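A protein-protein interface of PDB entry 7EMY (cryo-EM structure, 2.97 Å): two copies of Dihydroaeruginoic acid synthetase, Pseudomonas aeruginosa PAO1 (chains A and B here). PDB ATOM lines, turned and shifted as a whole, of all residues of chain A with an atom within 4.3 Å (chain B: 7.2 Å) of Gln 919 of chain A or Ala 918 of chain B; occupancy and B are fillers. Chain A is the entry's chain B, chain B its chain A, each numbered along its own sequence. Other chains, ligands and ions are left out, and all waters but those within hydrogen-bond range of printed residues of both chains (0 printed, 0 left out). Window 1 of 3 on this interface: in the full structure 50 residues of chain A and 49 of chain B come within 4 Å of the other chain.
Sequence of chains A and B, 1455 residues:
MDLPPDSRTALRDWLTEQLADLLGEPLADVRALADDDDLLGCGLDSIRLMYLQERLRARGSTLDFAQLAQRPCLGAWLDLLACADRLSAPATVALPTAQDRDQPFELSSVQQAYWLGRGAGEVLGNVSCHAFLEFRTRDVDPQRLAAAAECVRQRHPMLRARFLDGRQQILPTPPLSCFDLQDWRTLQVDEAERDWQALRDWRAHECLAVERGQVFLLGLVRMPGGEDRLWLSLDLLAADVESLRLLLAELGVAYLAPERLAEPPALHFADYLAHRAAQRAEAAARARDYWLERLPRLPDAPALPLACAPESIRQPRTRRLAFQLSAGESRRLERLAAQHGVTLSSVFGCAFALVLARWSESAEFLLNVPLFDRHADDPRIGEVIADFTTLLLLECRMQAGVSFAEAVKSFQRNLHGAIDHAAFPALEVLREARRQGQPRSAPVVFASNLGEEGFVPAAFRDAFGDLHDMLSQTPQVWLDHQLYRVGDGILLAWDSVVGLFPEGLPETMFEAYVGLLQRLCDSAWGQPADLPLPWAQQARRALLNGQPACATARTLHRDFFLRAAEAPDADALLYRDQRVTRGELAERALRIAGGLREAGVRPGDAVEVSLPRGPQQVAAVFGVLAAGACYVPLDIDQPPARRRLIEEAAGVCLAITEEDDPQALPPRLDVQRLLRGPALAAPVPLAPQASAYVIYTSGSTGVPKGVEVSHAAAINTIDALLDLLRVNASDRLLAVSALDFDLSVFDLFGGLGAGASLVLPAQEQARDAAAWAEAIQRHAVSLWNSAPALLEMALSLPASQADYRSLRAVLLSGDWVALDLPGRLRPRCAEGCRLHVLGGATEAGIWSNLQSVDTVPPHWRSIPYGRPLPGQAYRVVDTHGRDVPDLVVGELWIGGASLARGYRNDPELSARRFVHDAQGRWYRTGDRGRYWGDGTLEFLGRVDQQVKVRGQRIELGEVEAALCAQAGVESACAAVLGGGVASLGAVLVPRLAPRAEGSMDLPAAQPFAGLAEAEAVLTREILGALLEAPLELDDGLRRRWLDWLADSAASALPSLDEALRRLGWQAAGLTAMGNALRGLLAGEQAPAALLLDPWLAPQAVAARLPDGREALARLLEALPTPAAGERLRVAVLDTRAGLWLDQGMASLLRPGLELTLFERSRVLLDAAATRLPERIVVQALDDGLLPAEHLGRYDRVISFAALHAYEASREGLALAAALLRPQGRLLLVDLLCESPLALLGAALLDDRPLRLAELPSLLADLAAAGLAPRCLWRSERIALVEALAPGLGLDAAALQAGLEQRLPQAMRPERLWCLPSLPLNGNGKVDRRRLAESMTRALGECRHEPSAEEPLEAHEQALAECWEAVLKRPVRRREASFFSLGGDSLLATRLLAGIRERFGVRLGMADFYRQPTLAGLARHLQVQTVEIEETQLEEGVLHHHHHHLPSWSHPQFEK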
ATOM      1  N   ARG A 875       0.990 -21.546  20.019  1.00  0.00           N
ATOM      2  CA  ARG A 875       0.359 -22.803  19.986  1.00  0.00           C
ATOM      3  C   ARG A 875      -0.328 -23.155  21.275  1.00  0.00           C
ATOM      4  O   ARG A 875       0.312 -23.110  22.329  1.00  0.00           O
ATOM      5  CB  ARG A 875       1.207 -23.873  19.449  1.00  0.00           C
ATOM      6  CG  ARG A 875       1.616 -23.980  18.087  1.00  0.00           C
ATOM      7  CD  ARG A 875       2.522 -25.032  17.777  1.00  0.00           C
ATOM      8  NE  ARG A 875       2.125 -26.340  17.998  1.00  0.00           N
ATOM      9  CZ  ARG A 875       2.777 -27.452  18.099  1.00  0.00           C
ATOM     10  NH1 ARG A 875       3.993 -27.434  17.948  1.00  0.00           N
ATOM     11  NH2 ARG A 875       2.213 -28.523  18.331  1.00  0.00           N
ATOM     12  N   ASP A 883      -1.867 -29.680  19.131  1.00  0.00           N
ATOM     13  CA  ASP A 883      -2.591 -28.470  19.099  1.00  0.00           C
ATOM     14  C   ASP A 883      -4.038 -28.695  19.439  1.00  0.00           C
ATOM     15  O   ASP A 883      -4.648 -29.611  18.878  1.00  0.00           O
ATOM     16  CB  ASP A 883      -2.364 -27.682  17.886  1.00  0.00           C
ATOM     17  CG  ASP A 883      -0.985 -27.349  17.500  1.00  0.00           C
ATOM     18  OD1 ASP A 883      -0.093 -27.743  18.280  1.00  0.00           O
ATOM     19  OD2 ASP A 883      -0.742 -26.713  16.454  1.00  0.00           O
ATOM     20  N   ASP A 917       8.950 -29.609  17.671  1.00  0.00           N
ATOM     21  CA  ASP A 917       7.907 -30.167  16.908  1.00  0.00           C
ATOM     22  C   ASP A 917       8.131 -30.009  15.430  1.00  0.00           C
ATOM     23  O   ASP A 917       9.042 -29.285  15.019  1.00  0.00           O
ATOM     24  CB  ASP A 917       6.558 -29.762  17.334  1.00  0.00           C
ATOM     25  CG  ASP A 917       5.402 -30.609  16.993  1.00  0.00           C
ATOM     26  OD1 ASP A 917       5.545 -31.369  16.013  1.00  0.00           O
ATOM     27  OD2 ASP A 917       4.354 -30.568  17.673  1.00  0.00           O
ATOM     28  N   ALA A 918       7.286 -30.644  14.617  1.00  0.00           N
ATOM     29  CA  ALA A 918       7.348 -30.406  13.181  1.00  0.00           C
ATOM     30  C   ALA A 918       7.060 -28.947  12.855  1.00  0.00           C
ATOM     31  O   ALA A 918       7.401 -28.475  11.764  1.00  0.00           O
ATOM     32  CB  ALA A 918       6.367 -31.324  12.453  1.00  0.00           C
ATOM     33  N   GLN A 919       6.460 -28.195  13.717  1.00  0.00           N
ATOM     34  CA  GLN A 919       6.175 -26.812  13.672  1.00  0.00           C
ATOM     35  C   GLN A 919       7.303 -25.936  14.147  1.00  0.00           C
ATOM     36  O   GLN A 919       7.207 -24.704  14.119  1.00  0.00           O
ATOM     37  CB  GLN A 919       4.865 -26.482  14.248  1.00  0.00           C
ATOM     38  CG  GLN A 919       3.658 -27.160  13.874  1.00  0.00           C
ATOM     39  CD  GLN A 919       2.357 -26.720  14.400  1.00  0.00           C
ATOM     40  OE1 GLN A 919       2.170 -25.519  14.589  1.00  0.00           O
ATOM     41  NE2 GLN A 919       1.511 -27.573  14.668  1.00  0.00           N
ATOM     42  N   GLY A 920       8.367 -26.484  14.628  1.00  0.00           N
ATOM     43  CA  GLY A 920       9.491 -25.853  15.112  1.00  0.00           C
ATOM     44  C   GLY A 920       9.778 -25.865  16.559  1.00  0.00           C
ATOM     45  O   GLY A 920       9.450 -26.847  17.230  1.00  0.00           O
ATOM     46  N   TRP A 922       9.306 -24.299  20.420  1.00  0.00           N
ATOM     47  CA  TRP A 922       8.289 -23.804  21.261  1.00  0.00           C
ATOM     48  C   TRP A 922       8.650 -23.773  22.720  1.00  0.00           C
ATOM     49  O   TRP A 922       9.230 -24.747  23.208  1.00  0.00           O
ATOM     50  CB  TRP A 922       6.995 -24.423  20.948  1.00  0.00           C
ATOM     51  CG  TRP A 922       6.565 -24.461  19.564  1.00  0.00           C
ATOM     52  CD1 TRP A 922       6.840 -25.345  18.621  1.00  0.00           C
ATOM     53  CD2 TRP A 922       5.812 -23.458  18.875  1.00  0.00           C
ATOM     54  NE1 TRP A 922       6.357 -25.020  17.475  1.00  0.00           N
ATOM     55  CE2 TRP A 922       5.705 -23.866  17.533  1.00  0.00           C
ATOM     56  CE3 TRP A 922       5.211 -22.281  19.193  1.00  0.00           C
ATOM     57  CZ2 TRP A 922       5.029 -23.095  16.650  1.00  0.00           C
ATOM     58  CZ3 TRP A 922       4.574 -21.580  18.295  1.00  0.00           C
ATOM     59  CH2 TRP A 922       4.488 -21.992  17.040  1.00  0.00           C
ATOM     60  N   PRO B 532      14.462 -26.995  13.250  1.00  0.00           N
ATOM     61  CA  PRO B 532      13.352 -26.181  12.825  1.00  0.00           C
ATOM     62  C   PRO B 532      13.644 -25.426  11.562  1.00  0.00           C
ATOM     63  O   PRO B 532      14.794 -25.051  11.323  1.00  0.00           O
ATOM     64  CB  PRO B 532      13.101 -25.322  13.982  1.00  0.00           C
ATOM     65  CG  PRO B 532      14.336 -25.176  14.597  1.00  0.00           C
ATOM     66  CD  PRO B 532      15.025 -26.388  14.411  1.00  0.00           C
ATOM     67  N   LEU B 533      12.623 -25.173  10.749  1.00  0.00           N
ATOM     68  CA  LEU B 533      12.819 -24.312   9.603  1.00  0.00           C
ATOM     69  C   LEU B 533      13.187 -22.910  10.080  1.00  0.00           C
ATOM     70  O   LEU B 533      12.753 -22.477  11.150  1.00  0.00           O
ATOM     71  CB  LEU B 533      11.556 -24.250   8.748  1.00  0.00           C
ATOM     72  CG  LEU B 533      11.074 -25.541   8.091  1.00  0.00           C
ATOM     73  CD1 LEU B 533       9.927 -25.229   7.148  1.00  0.00           C
ATOM     74  CD2 LEU B 533      12.206 -26.225   7.352  1.00  0.00           C
ATOM     75  N   TRP B 535      12.544 -19.523  10.863  1.00  0.00           N
ATOM     76  CA  TRP B 535      11.256 -19.107  11.257  1.00  0.00           C
ATOM     77  C   TRP B 535      10.602 -18.227  10.228  1.00  0.00           C
ATOM     78  O   TRP B 535       9.377 -18.177  10.090  1.00  0.00           O
ATOM     79  CB  TRP B 535      11.092 -18.538  12.593  1.00  0.00           C
ATOM     80  CG  TRP B 535       9.755 -18.176  12.996  1.00  0.00           C
ATOM     81  CD1 TRP B 535       9.156 -16.999  13.012  1.00  0.00           C
ATOM     82  CD2 TRP B 535       8.719 -19.087  13.368  1.00  0.00           C
ATOM     83  NE1 TRP B 535       7.920 -17.074  13.353  1.00  0.00           N
ATOM     84  CE2 TRP B 535       7.558 -18.327  13.596  1.00  0.00           C
ATOM     85  CE3 TRP B 535       8.604 -20.430  13.557  1.00  0.00           C
ATOM     86  CZ2 TRP B 535       6.419 -18.947  13.975  1.00  0.00           C
ATOM     87  CZ3 TRP B 535       7.474 -20.967  13.928  1.00  0.00           C
ATOM     88  CH2 TRP B 535       6.396 -20.226  14.130  1.00  0.00           C
ATOM     89  N   GLN B 538       9.042 -20.726   7.704  1.00  0.00           N
ATOM     90  CA  GLN B 538       7.935 -21.330   8.334  1.00  0.00           C
ATOM     91  C   GLN B 538       6.760 -20.397   8.399  1.00  0.00           C
ATOM     92  O   GLN B 538       5.611 -20.760   8.139  1.00  0.00           O
ATOM     93  CB  GLN B 538       8.152 -21.990   9.626  1.00  0.00           C
ATOM     94  CG  GLN B 538       7.133 -22.763  10.272  1.00  0.00           C
ATOM     95  CD  GLN B 538       7.329 -23.290  11.627  1.00  0.00           C
ATOM     96  OE1 GLN B 538       8.478 -23.490  12.023  1.00  0.00           O
ATOM     97  NE2 GLN B 538       6.339 -23.487  12.332  1.00  0.00           N
ATOM     98  N   ARG B 875       2.800 -28.482   1.829  1.00  0.00           N
ATOM     99  CA  ARG B 875       3.970 -28.835   2.523  1.00  0.00           C
ATOM    100  C   ARG B 875       4.999 -29.502   1.655  1.00  0.00           C
ATOM    101  O   ARG B 875       4.674 -30.489   0.988  1.00  0.00           O
ATOM    102  CB  ARG B 875       3.717 -29.532   3.789  1.00  0.00           C
ATOM    103  CG  ARG B 875       3.143 -28.933   4.947  1.00  0.00           C
ATOM    104  CD  ARG B 875       2.880 -29.795   6.046  1.00  0.00           C
ATOM    105  NE  ARG B 875       3.937 -30.463   6.639  1.00  0.00           N
ATOM    106  CZ  ARG B 875       4.002 -31.491   7.420  1.00  0.00           C
ATOM    107  NH1 ARG B 875       2.958 -32.019   7.781  1.00  0.00           N
ATOM    108  NH2 ARG B 875       5.077 -31.946   7.816  1.00  0.00           N
ATOM    109  N   ASP B 883       9.220 -30.978   7.089  1.00  0.00           N
ATOM    110  CA  ASP B 883       9.178 -29.902   6.180  1.00  0.00           C
ATOM    111  C   ASP B 883      10.563 -29.491   5.763  1.00  0.00           C
ATOM    112  O   ASP B 883      11.423 -29.324   6.632  1.00  0.00           O
ATOM    113  CB  ASP B 883       8.316 -28.799   6.615  1.00  0.00           C
ATOM    114  CG  ASP B 883       6.923 -29.084   6.983  1.00  0.00           C
ATOM    115  OD1 ASP B 883       6.561 -30.272   6.854  1.00  0.00           O
ATOM    116  OD2 ASP B 883       6.166 -28.182   7.396  1.00  0.00           O
ATOM    117  N   HIS B 916      -0.902 -38.155   8.016  1.00  0.00           N
ATOM    118  CA  HIS B 916      -1.173 -37.286   9.088  1.00  0.00           C
ATOM    119  C   HIS B 916       0.059 -36.694   9.710  1.00  0.00           C
ATOM    120  O   HIS B 916       1.159 -37.229   9.541  1.00  0.00           O
ATOM    121  CB  HIS B 916      -2.128 -37.832  10.058  1.00  0.00           C
ATOM    122  CG  HIS B 916      -3.497 -38.110   9.665  1.00  0.00           C
ATOM    123  ND1 HIS B 916      -3.820 -39.173   8.850  1.00  0.00           N
ATOM    124  CD2 HIS B 916      -4.641 -37.498   9.841  1.00  0.00           C
ATOM    125  CE1 HIS B 916      -5.078 -39.098   8.637  1.00  0.00           C
ATOM    126  NE2 HIS B 916      -5.568 -38.123   9.210  1.00  0.00           N
ATOM    127  N   ASP B 917      -0.056 -35.648  10.452  1.00  0.00           N
ATOM    128  CA  ASP B 917       0.933 -34.928  11.145  1.00  0.00           C
ATOM    129  C   ASP B 917       0.348 -34.006  12.179  1.00  0.00           C
ATOM    130  O   ASP B 917      -0.870 -33.812  12.213  1.00  0.00           O
ATOM    131  CB  ASP B 917       1.926 -34.269  10.281  1.00  0.00           C
ATOM    132  CG  ASP B 917       3.250 -33.921  10.827  1.00  0.00           C
ATOM    133  OD1 ASP B 917       3.318 -33.793  12.066  1.00  0.00           O
ATOM    134  OD2 ASP B 917       4.238 -33.789  10.075  1.00  0.00           O
ATOM    135  N   ALA B 918       1.202 -33.398  13.003  1.00  0.00           N
ATOM    136  CA  ALA B 918       0.720 -32.374  13.919  1.00  0.00           C
ATOM    137  C   ALA B 918       0.125 -31.196  13.160  1.00  0.00           C
ATOM    138  O   ALA B 918      -0.637 -30.408  13.733  1.00  0.00           O
ATOM    139  CB  ALA B 918       1.853 -31.908  14.833  1.00  0.00           C
ATOM    140  N   GLN B 919       0.411 -31.015  11.913  1.00  0.00           N
ATOM    141  CA  GLN B 919      -0.086 -30.063  10.998  1.00  0.00           C
ATOM    142  C   GLN B 919      -1.372 -30.466  10.328  1.00  0.00           C
ATOM    143  O   GLN B 919      -1.944 -29.707   9.537  1.00  0.00           O
ATOM    144  CB  GLN B 919       0.946 -29.563  10.080  1.00  0.00           C
ATOM    145  CG  GLN B 919       2.216 -29.072  10.529  1.00  0.00           C
ATOM    146  CD  GLN B 919       3.173 -28.485   9.579  1.00  0.00           C
ATOM    147  OE1 GLN B 919       2.739 -27.835   8.628  1.00  0.00           O
ATOM    148  NE2 GLN B 919       4.372 -28.693   9.749  1.00  0.00           N
ATOM    149  N   GLY B 920      -1.860 -31.637  10.556  1.00  0.00           N
ATOM    150  CA  GLY B 920      -3.013 -32.181  10.038  1.00  0.00           C
ATOM    151  C   GLY B 920      -2.934 -33.269   9.043  1.00  0.00           C
ATOM    152  O   GLY B 920      -2.007 -34.079   9.109  1.00  0.00           O
ATOM    153  N   ARG B 921      -3.806 -33.359   8.097  1.00  0.00           N
ATOM    154  CA  ARG B 921      -3.939 -34.301   7.056  1.00  0.00           C
ATOM    155  C   ARG B 921      -3.296 -33.838   5.778  1.00  0.00           C
ATOM    156  O   ARG B 921      -3.523 -32.691   5.384  1.00  0.00           O
ATOM    157  CB  ARG B 921      -5.278 -34.841   6.796  1.00  0.00           C
ATOM    158  CG  ARG B 921      -5.507 -36.022   6.025  1.00  0.00           C
ATOM    159  CD  ARG B 921      -6.774 -36.292   5.416  1.00  0.00           C
ATOM    160  NE  ARG B 921      -7.050 -37.489   4.776  1.00  0.00           N
ATOM    161  CZ  ARG B 921      -7.995 -37.855   3.975  1.00  0.00           C
ATOM    162  NH1 ARG B 921      -8.838 -37.027   3.643  1.00  0.00           N
ATOM    163  NH2 ARG B 921      -8.066 -39.002   3.525  1.00  0.00           N
ATOM    164  N   TRP B 922      -2.535 -34.625   5.095  1.00  0.00           N
ATOM    165  CA  TRP B 922      -1.774 -34.357   3.939  1.00  0.00           C
ATOM    166  C   TRP B 922      -1.775 -35.466   2.925  1.00  0.00           C
ATOM    167  O   TRP B 922      -1.640 -36.628   3.316  1.00  0.00           O
ATOM    168  CB  TRP B 922      -0.450 -33.828   4.288  1.00  0.00           C
ATOM    169  CG  TRP B 922      -0.372 -32.735   5.238  1.00  0.00           C
ATOM    170  CD1 TRP B 922      -0.339 -32.768   6.558  1.00  0.00           C
ATOM    171  CD2 TRP B 922      -0.424 -31.337   4.938  1.00  0.00           C
ATOM    172  NE1 TRP B 922      -0.358 -31.598   7.088  1.00  0.00           N
ATOM    173  CE2 TRP B 922      -0.410 -30.647   6.164  1.00  0.00           C
ATOM    174  CE3 TRP B 922      -0.475 -30.568   3.818  1.00  0.00           C
ATOM    175  CZ2 TRP B 922      -0.443 -29.294   6.172  1.00  0.00           C
ATOM    176  CZ3 TRP B 922      -0.508 -29.265   3.892  1.00  0.00           C
ATOM    177  CH2 TRP B 922      -0.492 -28.643   5.060  1.00  0.00           C
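The side-chain amide oxygen (OE1) of Gln 538 of chain B sits close to the backbone carbonyl oxygen (O) of Gln 919 of chain A, at 2.7 Å.
NH2 of Arg 875 of chain B is in salt-bridge range of OD2 of Asp 917 of chain B.
The side-chain carboxylate (OD2) of Asp 883 of chain B sits at hydrogen-bond distance from the side-chain amide nitrogen (NE2) of Gln 919 of chain B.
The backbone carbonyl oxygen (O) of Gln 919 of chain B is in hydrogen-bond range of the indole nitrogen (NE1) of Trp 922 of chain B (3.5 Å).
The guanidinium group (NH2) of Arg 875 of chain A is in salt-bridge range of the side-chain carboxylate (OD2) of Asp 917 of chain A (3.0 Å).
The side-chain carboxylate (OD2) of Asp 883 of chain A sits at hydrogen-bond distance from the side-chain amide nitrogen (NE2) of Gln 919 of chain A.
The indole nitrogen (NE1) of Trp 922 of chain A sits at hydrogen-bond distance from the backbone carbonyl oxygen (O) of Gln 919 of chain A (3.5 Å).
Asp 917 of chain A touches Ala 918 of chain B.
Ala 918 of chain A touches Asp 917 of chain B (CB to OD1, 3.9 Å).
NE2 of Gln 919 of chain B touches O of Ala 918 of chain A, 3.6 Å away.
O of Gln 919 of chain A touches CZ3 of Trp 535 of chain B (3.8 Å).
O of Ala 918 of chain B touches NE2 of Gln 919 of chain A, at 3.7 Å.
Pro 532 of chain B touches Gly 920 of chain A.
Gly 920 of chain A touches Gln 538 of chain B (N to OE1, 3.97 Å).
Trp 535 of chain B touches Trp 922 of chain A (CH2 to CH2, 3.9 Å).
Gln 919 of chain A touches three residues of chain B.
Ala 918 of chain B touches two residues of chain A.
Printed residues of chain A within 4 Å of Gln 538 of chain B: Gln 919 and Gly 920.
Printed residues of chain A within 4 Å of Asp 917 of chain B: Ala 918 (3.9 Å).
Printed residues of chain B within 4 Å of Gly 920 of chain A: Pro 532 (3.8 Å) and Gln 538 (3.97 Å).
Of the printed residues of chain A, Trp 535 of chain B touches Gln 919 (3.8 Å) and Trp 922 (3.9 Å).
Leu 533 of chain B touches none of the printed residues of chain A.
His 916 of chain B touches none of the printed residues of chain A.
The nearest printed residue of chain A that does not touch Ala 918 of chain B is Asp 883 of chain A (4.6 Å).
Printed residues of chain A that touch a printed residue of chain B: Asp 917, Ala 918, Gln 919, Gly 920 and Trp 922.
Hydrophobic or aromatic side chains of chain A within 4 Å of the printed part of chain B: Ala 918 and Trp 922.
Of the 13 printed residues of chain B, 6 touch a printed residue of chain A.
Hydrophobic or aromatic side chains of chain B within 4 Å of the printed part of chain A: Pro 532, Trp 535 and Ala 918.
Along chain B the printed residues that touch a printed residue of chain A span positions 532 to 919.
Among the printed residues, no Asp or Glu carboxylate lies within 4 Å of a Lys or Arg side-chain nitrogen of the other chain.
Asp 917 of chain A touches Ala 918 of chain B, and with the chains exchanged Ala 918 of chain A touches Asp 917 of chain B.
Ala 918 of chain A touches Gln 919 of chain B, and with the chains exchanged Gln 919 of chain A touches Ala 918 of chain B.
Positions printed for both chains: 875, 883, 917, 918, 919, 920 and 922.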
